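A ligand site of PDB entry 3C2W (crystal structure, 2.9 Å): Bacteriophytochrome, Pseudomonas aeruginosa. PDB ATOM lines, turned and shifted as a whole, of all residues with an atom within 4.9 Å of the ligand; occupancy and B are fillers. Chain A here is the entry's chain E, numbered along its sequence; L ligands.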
ATOM      1  N   LEU A   9      29.374   6.347 -34.154  1.00  0.00           N
ATOM      2  CA  LEU A   9      30.316   7.457 -34.105  1.00  0.00           C
ATOM      3  C   LEU A   9      30.375   8.293 -35.387  1.00  0.00           C
ATOM      4  O   LEU A   9      30.459   9.521 -35.326  1.00  0.00           O
ATOM      5  CB  LEU A   9      31.715   6.957 -33.732  1.00  0.00           C
ATOM      6  CG  LEU A   9      31.967   6.728 -32.231  1.00  0.00           C
ATOM      7  CD1 LEU A   9      31.636   7.997 -31.462  1.00  0.00           C
ATOM      8  CD2 LEU A   9      31.167   5.552 -31.693  1.00  0.00           C
ATOM      9  N   CYS A  12      27.086  10.308 -35.248  1.00  0.00           N
ATOM     10  CA  CYS A  12      26.745  11.063 -34.036  1.00  0.00           C
ATOM     11  C   CYS A  12      26.675  12.575 -34.295  1.00  0.00           C
ATOM     12  O   CYS A  12      26.054  13.321 -33.537  1.00  0.00           O
ATOM     13  CB  CYS A  12      27.729  10.766 -32.901  1.00  0.00           C
ATOM     14  SG  CYS A  12      29.138  11.925 -32.795  1.00  0.00           S
ATOM     15  N   GLU A  13      27.321  13.008 -35.378  1.00  0.00           N
ATOM     16  CA  GLU A  13      27.351  14.415 -35.752  1.00  0.00           C
ATOM     17  C   GLU A  13      25.967  14.904 -36.161  1.00  0.00           C
ATOM     18  O   GLU A  13      25.466  15.895 -35.631  1.00  0.00           O
ATOM     19  CB  GLU A  13      28.320  14.618 -36.917  1.00  0.00           C
ATOM     20  CG  GLU A  13      29.641  13.888 -36.741  1.00  0.00           C
ATOM     21  CD  GLU A  13      30.541  14.008 -37.961  1.00  0.00           C
ATOM     22  OE1 GLU A  13      30.022  14.138 -39.082  1.00  0.00           O
ATOM     23  OE2 GLU A  13      31.775  13.960 -37.785  1.00  0.00           O
ATOM     24  N   ILE A  17      18.552  14.493 -32.618  1.00  0.00           N
ATOM     25  CA  ILE A  17      18.176  14.207 -31.235  1.00  0.00           C
ATOM     26  C   ILE A  17      16.945  15.015 -30.823  1.00  0.00           C
ATOM     27  O   ILE A  17      16.544  14.998 -29.664  1.00  0.00           O
ATOM     28  CB  ILE A  17      19.316  14.493 -30.230  1.00  0.00           C
ATOM     29  CG1 ILE A  17      20.662  14.592 -30.962  1.00  0.00           C
ATOM     30  CG2 ILE A  17      19.332  13.443 -29.136  1.00  0.00           C
ATOM     31  CD1 ILE A  17      20.950  15.978 -31.527  1.00  0.00           C
ATOM     32  N   TYR A 163      31.057  25.209 -17.499  1.00  0.00           N
ATOM     33  CA  TYR A 163      31.874  25.241 -18.696  1.00  0.00           C
ATOM     34  C   TYR A 163      31.904  26.645 -19.266  1.00  0.00           C
ATOM     35  O   TYR A 163      30.920  27.381 -19.170  1.00  0.00           O
ATOM     36  CB  TYR A 163      31.324  24.287 -19.757  1.00  0.00           C
ATOM     37  CG  TYR A 163      31.037  22.873 -19.284  1.00  0.00           C
ATOM     38  CD1 TYR A 163      29.736  22.412 -19.196  1.00  0.00           C
ATOM     39  CD2 TYR A 163      32.071  22.017 -18.928  1.00  0.00           C
ATOM     40  CE1 TYR A 163      29.465  21.127 -18.765  1.00  0.00           C
ATOM     41  CE2 TYR A 163      31.816  20.728 -18.504  1.00  0.00           C
ATOM     42  CZ  TYR A 163      30.503  20.293 -18.430  1.00  0.00           C
ATOM     43  OH  TYR A 163      30.249  19.017 -17.995  1.00  0.00           O
ATOM     44  N   TYR A 185      37.220  17.060 -12.546  1.00  0.00           N
ATOM     45  CA  TYR A 185      37.332  17.307 -13.975  1.00  0.00           C
ATOM     46  C   TYR A 185      37.750  18.747 -14.261  1.00  0.00           C
ATOM     47  O   TYR A 185      37.630  19.210 -15.398  1.00  0.00           O
ATOM     48  CB  TYR A 185      36.015  17.024 -14.685  1.00  0.00           C
ATOM     49  CG  TYR A 185      35.553  15.580 -14.659  1.00  0.00           C
ATOM     50  CD1 TYR A 185      35.978  14.686 -15.626  1.00  0.00           C
ATOM     51  CD2 TYR A 185      34.682  15.129 -13.685  1.00  0.00           C
ATOM     52  CE1 TYR A 185      35.551  13.365 -15.606  1.00  0.00           C
ATOM     53  CE2 TYR A 185      34.248  13.817 -13.657  1.00  0.00           C
ATOM     54  CZ  TYR A 185      34.685  12.941 -14.622  1.00  0.00           C
ATOM     55  OH  TYR A 185      34.248  11.629 -14.585  1.00  0.00           O
ATOM     56  N   GLN A 188      39.507  20.690 -17.573  1.00  0.00           N
ATOM     57  CA  GLN A 188      39.243  19.710 -18.622  1.00  0.00           C
ATOM     58  C   GLN A 188      38.897  20.399 -19.929  1.00  0.00           C
ATOM     59  O   GLN A 188      38.034  21.281 -19.963  1.00  0.00           O
ATOM     60  CB  GLN A 188      38.104  18.774 -18.213  1.00  0.00           C
ATOM     61  CG  GLN A 188      37.623  17.861 -19.320  1.00  0.00           C
ATOM     62  CD  GLN A 188      38.624  16.768 -19.645  1.00  0.00           C
ATOM     63  OE1 GLN A 188      39.137  16.082 -18.759  1.00  0.00           O
ATOM     64  NE2 GLN A 188      38.899  16.588 -20.931  1.00  0.00           N
ATOM     65  N   TYR A 190      37.443  19.536 -23.471  1.00  0.00           N
ATOM     66  CA  TYR A 190      36.813  18.645 -24.452  1.00  0.00           C
ATOM     67  C   TYR A 190      36.472  19.397 -25.741  1.00  0.00           C
ATOM     68  O   TYR A 190      36.274  20.613 -25.711  1.00  0.00           O
ATOM     69  CB  TYR A 190      35.576  17.979 -23.853  1.00  0.00           C
ATOM     70  CG  TYR A 190      34.492  18.936 -23.389  1.00  0.00           C
ATOM     71  CD1 TYR A 190      34.322  19.219 -22.050  1.00  0.00           C
ATOM     72  CD2 TYR A 190      33.643  19.559 -24.297  1.00  0.00           C
ATOM     73  CE1 TYR A 190      33.337  20.086 -21.618  1.00  0.00           C
ATOM     74  CE2 TYR A 190      32.651  20.420 -23.877  1.00  0.00           C
ATOM     75  CZ  TYR A 190      32.514  20.687 -22.539  1.00  0.00           C
ATOM     76  OH  TYR A 190      31.526  21.547 -22.129  1.00  0.00           O
ATOM     77  N   SER A 193      33.382  18.615 -30.886  1.00  0.00           N
ATOM     78  CA  SER A 193      32.670  17.418 -31.338  1.00  0.00           C
ATOM     79  C   SER A 193      31.698  16.954 -30.256  1.00  0.00           C
ATOM     80  O   SER A 193      30.537  16.663 -30.543  1.00  0.00           O
ATOM     81  CB  SER A 193      33.659  16.306 -31.665  1.00  0.00           C
ATOM     82  OG  SER A 193      34.707  16.779 -32.490  1.00  0.00           O
ATOM     83  N   ASP A 194      32.183  16.897 -29.022  1.00  0.00           N
ATOM     84  CA  ASP A 194      31.389  16.399 -27.903  1.00  0.00           C
ATOM     85  C   ASP A 194      30.038  17.092 -27.754  1.00  0.00           C
ATOM     86  O   ASP A 194      29.166  16.604 -27.038  1.00  0.00           O
ATOM     87  CB  ASP A 194      32.182  16.514 -26.598  1.00  0.00           C
ATOM     88  CG  ASP A 194      33.202  15.396 -26.430  1.00  0.00           C
ATOM     89  OD1 ASP A 194      34.107  15.544 -25.593  1.00  0.00           O
ATOM     90  OD2 ASP A 194      33.076  14.372 -27.142  1.00  0.00           O
ATOM     91  N   ILE A 195      29.875  18.236 -28.405  1.00  0.00           N
ATOM     92  CA  ILE A 195      28.584  18.903 -28.446  1.00  0.00           C
ATOM     93  C   ILE A 195      28.264  19.302 -29.890  1.00  0.00           C
ATOM     94  O   ILE A 195      28.769  20.308 -30.403  1.00  0.00           O
ATOM     95  CB  ILE A 195      28.541  20.142 -27.509  1.00  0.00           C
ATOM     96  CG1 ILE A 195      28.512  19.704 -26.050  1.00  0.00           C
ATOM     97  CG2 ILE A 195      27.325  20.979 -27.797  1.00  0.00           C
ATOM     98  CD1 ILE A 195      28.231  20.830 -25.076  1.00  0.00           C
ATOM     99  N   PRO A 196      27.425  18.481 -30.556  1.00  0.00           N
ATOM    100  CA  PRO A 196      27.071  18.611 -31.976  1.00  0.00           C
ATOM    101  C   PRO A 196      26.135  19.776 -32.269  1.00  0.00           C
ATOM    102  O   PRO A 196      25.302  20.130 -31.434  1.00  0.00           O
ATOM    103  CB  PRO A 196      26.356  17.279 -32.278  1.00  0.00           C
ATOM    104  CG  PRO A 196      26.676  16.375 -31.122  1.00  0.00           C
ATOM    105  CD  PRO A 196      26.836  17.284 -29.953  1.00  0.00           C
ATOM    106  N   ALA A 199      22.651  19.588 -30.947  1.00  0.00           N
ATOM    107  CA  ALA A 199      22.445  19.453 -29.505  1.00  0.00           C
ATOM    108  C   ALA A 199      22.721  20.797 -28.831  1.00  0.00           C
ATOM    109  O   ALA A 199      22.022  21.187 -27.892  1.00  0.00           O
ATOM    110  CB  ALA A 199      23.346  18.378 -28.937  1.00  0.00           C
ATOM    111  N   TYR A 203      20.658  23.647 -26.552  1.00  0.00           N
ATOM    112  CA  TYR A 203      21.060  24.233 -25.286  1.00  0.00           C
ATOM    113  C   TYR A 203      20.848  25.745 -25.241  1.00  0.00           C
ATOM    114  O   TYR A 203      20.804  26.337 -24.172  1.00  0.00           O
ATOM    115  CB  TYR A 203      22.508  23.868 -24.958  1.00  0.00           C
ATOM    116  CG  TYR A 203      22.652  22.517 -24.304  1.00  0.00           C
ATOM    117  CD1 TYR A 203      23.785  21.744 -24.485  1.00  0.00           C
ATOM    118  CD2 TYR A 203      21.627  22.009 -23.492  1.00  0.00           C
ATOM    119  CE1 TYR A 203      23.906  20.511 -23.883  1.00  0.00           C
ATOM    120  CE2 TYR A 203      21.740  20.770 -22.892  1.00  0.00           C
ATOM    121  CZ  TYR A 203      22.883  20.024 -23.081  1.00  0.00           C
ATOM    122  OH  TYR A 203      23.000  18.799 -22.481  1.00  0.00           O
ATOM    123  N   ARG A 209      17.724  21.904 -19.294  1.00  0.00           N
ATOM    124  CA  ARG A 209      17.470  20.573 -19.839  1.00  0.00           C
ATOM    125  C   ARG A 209      17.699  19.511 -18.762  1.00  0.00           C
ATOM    126  O   ARG A 209      18.751  19.493 -18.129  1.00  0.00           O
ATOM    127  CB  ARG A 209      18.370  20.312 -21.053  1.00  0.00           C
ATOM    128  CG  ARG A 209      18.346  18.859 -21.513  1.00  0.00           C
ATOM    129  CD  ARG A 209      16.930  18.417 -21.848  1.00  0.00           C
ATOM    130  NE  ARG A 209      16.845  16.998 -22.129  1.00  0.00           N
ATOM    131  CZ  ARG A 209      17.309  16.411 -23.234  1.00  0.00           C
ATOM    132  NH1 ARG A 209      17.903  17.147 -24.157  1.00  0.00           N
ATOM    133  NH2 ARG A 209      17.188  15.108 -23.405  1.00  0.00           N
ATOM    134  N   ILE A 211      17.598  15.409 -17.545  1.00  0.00           N
ATOM    135  CA  ILE A 211      17.502  13.967 -17.723  1.00  0.00           C
ATOM    136  C   ILE A 211      17.346  13.338 -16.351  1.00  0.00           C
ATOM    137  O   ILE A 211      18.265  13.409 -15.528  1.00  0.00           O
ATOM    138  CB  ILE A 211      18.778  13.402 -18.393  1.00  0.00           C
ATOM    139  CG1 ILE A 211      19.118  14.214 -19.643  1.00  0.00           C
ATOM    140  CG2 ILE A 211      18.619  11.931 -18.731  1.00  0.00           C
ATOM    141  CD1 ILE A 211      20.421  13.803 -20.313  1.00  0.00           C
ATOM    142  N   ARG A 241      11.680  14.983 -23.807  1.00  0.00           N
ATOM    143  CA  ARG A 241      12.355  14.452 -24.994  1.00  0.00           C
ATOM    144  C   ARG A 241      13.505  13.494 -24.667  1.00  0.00           C
ATOM    145  O   ARG A 241      14.309  13.747 -23.767  1.00  0.00           O
ATOM    146  CB  ARG A 241      12.860  15.613 -25.856  1.00  0.00           C
ATOM    147  CG  ARG A 241      13.985  15.257 -26.821  1.00  0.00           C
ATOM    148  CD  ARG A 241      14.374  16.463 -27.663  1.00  0.00           C
ATOM    149  NE  ARG A 241      14.378  17.709 -26.889  1.00  0.00           N
ATOM    150  CZ  ARG A 241      15.472  18.261 -26.373  1.00  0.00           C
ATOM    151  NH1 ARG A 241      15.386  19.394 -25.690  1.00  0.00           N
ATOM    152  NH2 ARG A 241      16.651  17.687 -26.550  1.00  0.00           N
ATOM    153  N   SER A 242      13.576  12.388 -25.406  1.00  0.00           N
ATOM    154  CA  SER A 242      14.583  11.359 -25.153  1.00  0.00           C
ATOM    155  C   SER A 242      16.002  11.858 -25.388  1.00  0.00           C
ATOM    156  O   SER A 242      16.229  12.819 -26.126  1.00  0.00           O
ATOM    157  CB  SER A 242      14.326  10.109 -26.002  1.00  0.00           C
ATOM    158  OG  SER A 242      14.694  10.316 -27.353  1.00  0.00           O
ATOM    159  N   VAL A 243      16.957  11.185 -24.751  1.00  0.00           N
ATOM    160  CA  VAL A 243      18.362  11.538 -24.858  1.00  0.00           C
ATOM    161  C   VAL A 243      19.059  10.675 -25.902  1.00  0.00           C
ATOM    162  O   VAL A 243      18.652   9.538 -26.133  1.00  0.00           O
ATOM    163  CB  VAL A 243      19.063  11.368 -23.502  1.00  0.00           C
ATOM    164  CG1 VAL A 243      20.456  11.979 -23.552  1.00  0.00           C
ATOM    165  CG2 VAL A 243      18.242  12.013 -22.388  1.00  0.00           C
ATOM    166  N   SER A 244      20.094  11.213 -26.527  1.00  0.00           N
ATOM    167  CA  SER A 244      20.860  10.426 -27.494  1.00  0.00           C
ATOM    168  C   SER A 244      21.459   9.188 -26.841  1.00  0.00           C
ATOM    169  O   SER A 244      22.032   9.279 -25.757  1.00  0.00           O
ATOM    170  CB  SER A 244      21.974  11.286 -28.113  1.00  0.00           C
ATOM    171  OG  SER A 244      22.660  10.565 -29.113  1.00  0.00           O
ATOM    172  N   ILE A 246      23.992   7.618 -27.628  1.00  0.00           N
ATOM    173  CA  ILE A 246      25.441   7.750 -27.560  1.00  0.00           C
ATOM    174  C   ILE A 246      25.858   8.515 -26.308  1.00  0.00           C
ATOM    175  O   ILE A 246      26.826   8.145 -25.639  1.00  0.00           O
ATOM    176  CB  ILE A 246      25.996   8.461 -28.813  1.00  0.00           C
ATOM    177  CG1 ILE A 246      26.065   7.491 -29.993  1.00  0.00           C
ATOM    178  CG2 ILE A 246      27.361   9.027 -28.527  1.00  0.00           C
ATOM    179  CD1 ILE A 246      26.993   6.308 -29.774  1.00  0.00           C
ATOM    180  N   HIS A 247      25.114   9.576 -25.988  1.00  0.00           N
ATOM    181  CA  HIS A 247      25.363  10.366 -24.790  1.00  0.00           C
ATOM    182  C   HIS A 247      24.996   9.576 -23.527  1.00  0.00           C
ATOM    183  O   HIS A 247      25.552   9.818 -22.454  1.00  0.00           O
ATOM    184  CB  HIS A 247      24.567  11.677 -24.835  1.00  0.00           C
ATOM    185  CG  HIS A 247      24.779  12.550 -23.641  1.00  0.00           C
ATOM    186  ND1 HIS A 247      25.769  13.514 -23.583  1.00  0.00           N
ATOM    187  CD2 HIS A 247      24.125  12.628 -22.459  1.00  0.00           C
ATOM    188  CE1 HIS A 247      25.720  14.120 -22.423  1.00  0.00           C
ATOM    189  NE2 HIS A 247      24.723  13.607 -21.717  1.00  0.00           N
ATOM    190  N   TYR A 250      27.784   7.389 -22.599  1.00  0.00           N
ATOM    191  CA  TYR A 250      28.808   8.267 -22.053  1.00  0.00           C
ATOM    192  C   TYR A 250      28.638   8.362 -20.540  1.00  0.00           C
ATOM    193  O   TYR A 250      29.532   7.980 -19.776  1.00  0.00           O
ATOM    194  CB  TYR A 250      28.750   9.659 -22.676  1.00  0.00           C
ATOM    195  CG  TYR A 250      30.033  10.448 -22.504  1.00  0.00           C
ATOM    196  CD1 TYR A 250      30.517  10.755 -21.235  1.00  0.00           C
ATOM    197  CD2 TYR A 250      30.754  10.898 -23.599  1.00  0.00           C
ATOM    198  CE1 TYR A 250      31.674  11.475 -21.061  1.00  0.00           C
ATOM    199  CE2 TYR A 250      31.920  11.630 -23.444  1.00  0.00           C
ATOM    200  CZ  TYR A 250      32.373  11.909 -22.171  1.00  0.00           C
ATOM    201  OH  TYR A 250      33.541  12.633 -22.005  1.00  0.00           O
ATOM    202  N   LEU A 251      27.488   8.870 -20.115  1.00  0.00           N
ATOM    203  CA  LEU A 251      27.255   9.087 -18.696  1.00  0.00           C
ATOM    204  C   LEU A 251      27.382   7.803 -17.883  1.00  0.00           C
ATOM    205  O   LEU A 251      28.059   7.780 -16.850  1.00  0.00           O
ATOM    206  CB  LEU A 251      25.893   9.744 -18.455  1.00  0.00           C
ATOM    207  CG  LEU A 251      25.618  11.016 -19.264  1.00  0.00           C
ATOM    208  CD1 LEU A 251      24.469  11.812 -18.665  1.00  0.00           C
ATOM    209  CD2 LEU A 251      26.867  11.878 -19.342  1.00  0.00           C
ATOM    210  N   MET A 254      30.891   7.181 -17.230  1.00  0.00           N
ATOM    211  CA  MET A 254      31.312   8.096 -16.180  1.00  0.00           C
ATOM    212  C   MET A 254      30.682   7.704 -14.857  1.00  0.00           C
ATOM    213  O   MET A 254      31.018   8.247 -13.813  1.00  0.00           O
ATOM    214  CB  MET A 254      30.928   9.532 -16.528  1.00  0.00           C
ATOM    215  CG  MET A 254      31.892  10.243 -17.447  1.00  0.00           C
ATOM    216  SD  MET A 254      31.384  11.938 -17.776  1.00  0.00           S
ATOM    217  CE  MET A 254      31.214  12.571 -16.111  1.00  0.00           C
ATOM    218  N   SER A 259      21.011  14.254 -15.053  1.00  0.00           N
ATOM    219  CA  SER A 259      21.565  15.454 -15.666  1.00  0.00           C
ATOM    220  C   SER A 259      20.600  16.628 -15.759  1.00  0.00           C
ATOM    221  O   SER A 259      19.430  16.481 -16.116  1.00  0.00           O
ATOM    222  CB  SER A 259      22.128  15.126 -17.046  1.00  0.00           C
ATOM    223  OG  SER A 259      22.336  16.290 -17.819  1.00  0.00           O
ATOM    224  N   SER A 275      26.603  22.272 -15.615  1.00  0.00           N
ATOM    225  CA  SER A 275      26.159  20.877 -15.690  1.00  0.00           C
ATOM    226  C   SER A 275      26.153  20.214 -14.318  1.00  0.00           C
ATOM    227  O   SER A 275      27.117  20.334 -13.558  1.00  0.00           O
ATOM    228  CB  SER A 275      27.044  20.087 -16.657  1.00  0.00           C
ATOM    229  OG  SER A 275      26.675  18.721 -16.672  1.00  0.00           O
ATOM    230  N   HIS A 277      25.603  16.587 -12.389  1.00  0.00           N
ATOM    231  CA  HIS A 277      25.429  15.133 -12.402  1.00  0.00           C
ATOM    232  C   HIS A 277      25.050  14.577 -11.028  1.00  0.00           C
ATOM    233  O   HIS A 277      25.301  15.209  -9.999  1.00  0.00           O
ATOM    234  CB  HIS A 277      26.683  14.453 -12.938  1.00  0.00           C
ATOM    235  CG  HIS A 277      27.133  14.989 -14.261  1.00  0.00           C
ATOM    236  ND1 HIS A 277      28.456  15.026 -14.635  1.00  0.00           N
ATOM    237  CD2 HIS A 277      26.429  15.531 -15.283  1.00  0.00           C
ATOM    238  CE1 HIS A 277      28.547  15.567 -15.855  1.00  0.00           C
ATOM    239  NE2 HIS A 277      27.338  15.877 -16.252  1.00  0.00           N
ATOM    240  N   ARG A 453      36.544   6.104 -26.806  1.00  0.00           N
ATOM    241  CA  ARG A 453      36.508   7.521 -27.177  1.00  0.00           C
ATOM    242  C   ARG A 453      35.364   8.240 -26.449  1.00  0.00           C
ATOM    243  O   ARG A 453      35.231   9.456 -26.547  1.00  0.00           O
ATOM    244  CB  ARG A 453      36.353   7.674 -28.692  1.00  0.00           C
ATOM    245  CG  ARG A 453      36.734   9.043 -29.253  1.00  0.00           C
ATOM    246  CD  ARG A 453      35.626  10.051 -29.065  1.00  0.00           C
ATOM    247  NE  ARG A 453      35.859  11.295 -29.794  1.00  0.00           N
ATOM    248  CZ  ARG A 453      35.311  12.465 -29.469  1.00  0.00           C
ATOM    249  NH1 ARG A 453      34.517  12.548 -28.406  1.00  0.00           N
ATOM    250  NH2 ARG A 453      35.572  13.555 -30.173  1.00  0.00           N
ATOM    251  N   LEU A 454      34.567   7.482 -25.722  1.00  0.00           N
ATOM    252  CA  LEU A 454      33.347   8.019 -25.120  1.00  0.00           C
ATOM    253  C   LEU A 454      33.546   8.413 -23.659  1.00  0.00           C
ATOM    254  O   LEU A 454      32.583   8.652 -22.936  1.00  0.00           O
ATOM    255  CB  LEU A 454      32.238   6.978 -25.236  1.00  0.00           C
ATOM    256  CG  LEU A 454      30.813   7.341 -24.834  1.00  0.00           C
ATOM    257  CD1 LEU A 454      30.035   7.842 -26.049  1.00  0.00           C
ATOM    258  CD2 LEU A 454      30.152   6.119 -24.269  1.00  0.00           C
ATOM    259  N   PRO A 456      36.020  10.646 -20.462  1.00  0.00           N
ATOM    260  CA  PRO A 456      36.839  11.841 -20.210  1.00  0.00           C
ATOM    261  C   PRO A 456      38.216  11.762 -20.875  1.00  0.00           C
ATOM    262  O   PRO A 456      38.593  12.682 -21.593  1.00  0.00           O
ATOM    263  CB  PRO A 456      36.965  11.835 -18.689  1.00  0.00           C
ATOM    264  CG  PRO A 456      35.687  11.227 -18.217  1.00  0.00           C
ATOM    265  CD  PRO A 456      35.301  10.207 -19.254  1.00  0.00           C
ATOM    266  N   SER A 459      37.859  12.177 -24.603  1.00  0.00           N
ATOM    267  CA  SER A 459      37.477  13.519 -25.029  1.00  0.00           C
ATOM    268  C   SER A 459      38.700  14.403 -25.103  1.00  0.00           C
ATOM    269  O   SER A 459      38.851  15.206 -26.030  1.00  0.00           O
ATOM    270  CB  SER A 459      36.471  14.129 -24.054  1.00  0.00           C
ATOM    271  OG  SER A 459      35.297  13.334 -23.960  1.00  0.00           O
HETATM  272  C1  LIG L   1      25.950  16.828 -24.239  1.00  0.00           C
HETATM  273  N1  LIG L   1      28.301  16.205 -24.122  1.00  0.00           N
HETATM  274  C2  LIG L   1      27.242  16.889 -23.774  1.00  0.00           C
HETATM  275  C3  LIG L   1      27.555  17.603 -22.608  1.00  0.00           C
HETATM  276  C4  LIG L   1      28.918  17.397 -22.423  1.00  0.00           C
HETATM  277  C5  LIG L   1      29.369  16.473 -23.373  1.00  0.00           C
HETATM  278  C6  LIG L   1      29.740  18.050 -21.299  1.00  0.00           C
HETATM  279  C7  LIG L   1      26.635  18.576 -21.864  1.00  0.00           C
HETATM  280  C8  LIG L   1      25.756  17.971 -20.762  1.00  0.00           C
HETATM  281  C9  LIG L   1      26.566  17.374 -19.597  1.00  0.00           C
HETATM  282  O1  LIG L   1      26.183  16.272 -19.152  1.00  0.00           O
HETATM  283  O2  LIG L   1      27.526  18.052 -19.183  1.00  0.00           O
HETATM  284  C10 LIG L   1      30.760  15.845 -23.607  1.00  0.00           C
HETATM  285  N2  LIG L   1      33.049  15.963 -22.567  1.00  0.00           N
HETATM  286  C11 LIG L   1      31.740  15.751 -22.420  1.00  0.00           C
HETATM  287  C12 LIG L   1      31.520  15.403 -21.086  1.00  0.00           C
HETATM  288  C13 LIG L   1      32.736  15.444 -20.444  1.00  0.00           C
HETATM  289  C14 LIG L   1      33.675  15.796 -21.406  1.00  0.00           C
HETATM  290  C15 LIG L   1      30.190  15.046 -20.421  1.00  0.00           C
HETATM  291  O3  LIG L   1      34.885  15.930 -21.234  1.00  0.00           O
HETATM  292  C16 LIG L   1      32.988  15.175 -19.096  1.00  0.00           C
HETATM  293  C17 LIG L   1      34.285  15.256 -18.599  1.00  0.00           C
HETATM  294  N3  LIG L   1      28.214  13.062 -26.870  1.00  0.00           N
HETATM  295  C18 LIG L   1      29.381  12.462 -27.029  1.00  0.00           C
HETATM  296  C19 LIG L   1      29.639  12.295 -28.382  1.00  0.00           C
HETATM  297  C20 LIG L   1      28.568  12.847 -29.075  1.00  0.00           C
HETATM  298  C21 LIG L   1      27.697  13.303 -28.079  1.00  0.00           C
HETATM  299  C22 LIG L   1      30.909  11.656 -28.936  1.00  0.00           C
HETATM  300  O4  LIG L   1      30.128  12.094 -26.128  1.00  0.00           O
HETATM  301  C23 LIG L   1      28.302  12.949 -30.595  1.00  0.00           C
HETATM  302  C24 LIG L   1      29.550  12.873 -31.479  1.00  0.00           C
HETATM  303  C25 LIG L   1      26.366  13.987 -28.349  1.00  0.00           C
HETATM  304  N4  LIG L   1      26.517  15.415 -26.170  1.00  0.00           N
HETATM  305  C26 LIG L   1      25.843  14.829 -27.187  1.00  0.00           C
HETATM  306  C27 LIG L   1      24.523  15.132 -26.982  1.00  0.00           C
HETATM  307  C28 LIG L   1      24.427  15.927 -25.853  1.00  0.00           C
HETATM  308  C29 LIG L   1      25.676  16.088 -25.404  1.00  0.00           C
HETATM  309  C30 LIG L   1      23.369  14.671 -27.890  1.00  0.00           C
HETATM  310  C31 LIG L   1      23.065  16.467 -25.308  1.00  0.00           C
HETATM  311  C32 LIG L   1      22.157  15.279 -24.943  1.00  0.00           C
HETATM  312  C33 LIG L   1      20.794  15.702 -24.403  1.00  0.00           C
HETATM  313  O5  LIG L   1      19.820  15.520 -25.163  1.00  0.00           O
HETATM  314  O6  LIG L   1      20.736  16.187 -23.250  1.00  0.00           O
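Merely in contact with the ligand: Tyr 185, Gln 188, Tyr 190, Ile 195, Pro 196, Ala 199, Tyr 203, Ile 211, Val 243, Ser 244, Ile 246, Met 254, Arg 453 and Ser 459.
Hydrophobic or aromatic side chains that line the ligand: Tyr 163, Tyr 185, Tyr 190, Ile 195, Pro 196, Ala 199, Tyr 203, Ile 211, Val 243, Ile 246, His 247, Tyr 250, Met 254 and His 277.
Of the 32 residues printed, 22 come within 4 Å of the ligand.
The side-chain sulfur of Cys 12 is covalently linked to a carbon (C24) of the ligand (1.7 Å).
The guanidinium group (NH1) of Arg 209 lies within salt-bridge range of an oxygen (O5) of the ligand (2.7 Å).
O2 of the ligand lies within hydrogen-bond range of OG of Ser 275 (2.7 Å).
A nitrogen (N2) of the ligand sits close to the side-chain hydroxyl of Tyr 250 (3.4 Å).
O of Asp 194 is in hydrogen-bond range of N1 of the ligand, at 3.1 Å.
The side-chain carboxylate (OD1) of Asp 194 sits at hydrogen-bond distance from a nitrogen (N2) of the ligand.
The side-chain hydroxyl (OH) of Tyr 163 lies within hydrogen-bond range of an oxygen (O2) of the ligand, at 3.1 Å.
NE2 of His 277 sits at hydrogen-bond distance from O1 of the ligand, at 3.1 Å.
A nitrogen (N4) of the ligand lies close to a ring nitrogen (ND1) of His 247 (3.3 Å).
O of Arg 241 is in hydrogen-bond range of NH2 of Arg 209, 3.2 Å away.
The side-chain hydroxyl (OG) of Ser 275 is in hydrogen-bond range of a ring nitrogen (NE2) of His 277 (3.0 Å).
The side-chain hydroxyl (OG) of Ser 459 is in hydrogen-bond range of the side-chain hydroxyl (OH) of Tyr 250, at 2.7 Å.
The side-chain carboxylate of Asp 194 sits at hydrogen-bond distance from the side-chain hydroxyl of Ser 459, at 3.0 Å.
OD2 of Asp 194 is in salt-bridge range of NH1 of Arg 453.
The backbone NH (N) of Ile 211 sits at hydrogen-bond distance from the backbone carbonyl oxygen (O) of Ser 259 (2.6 Å).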
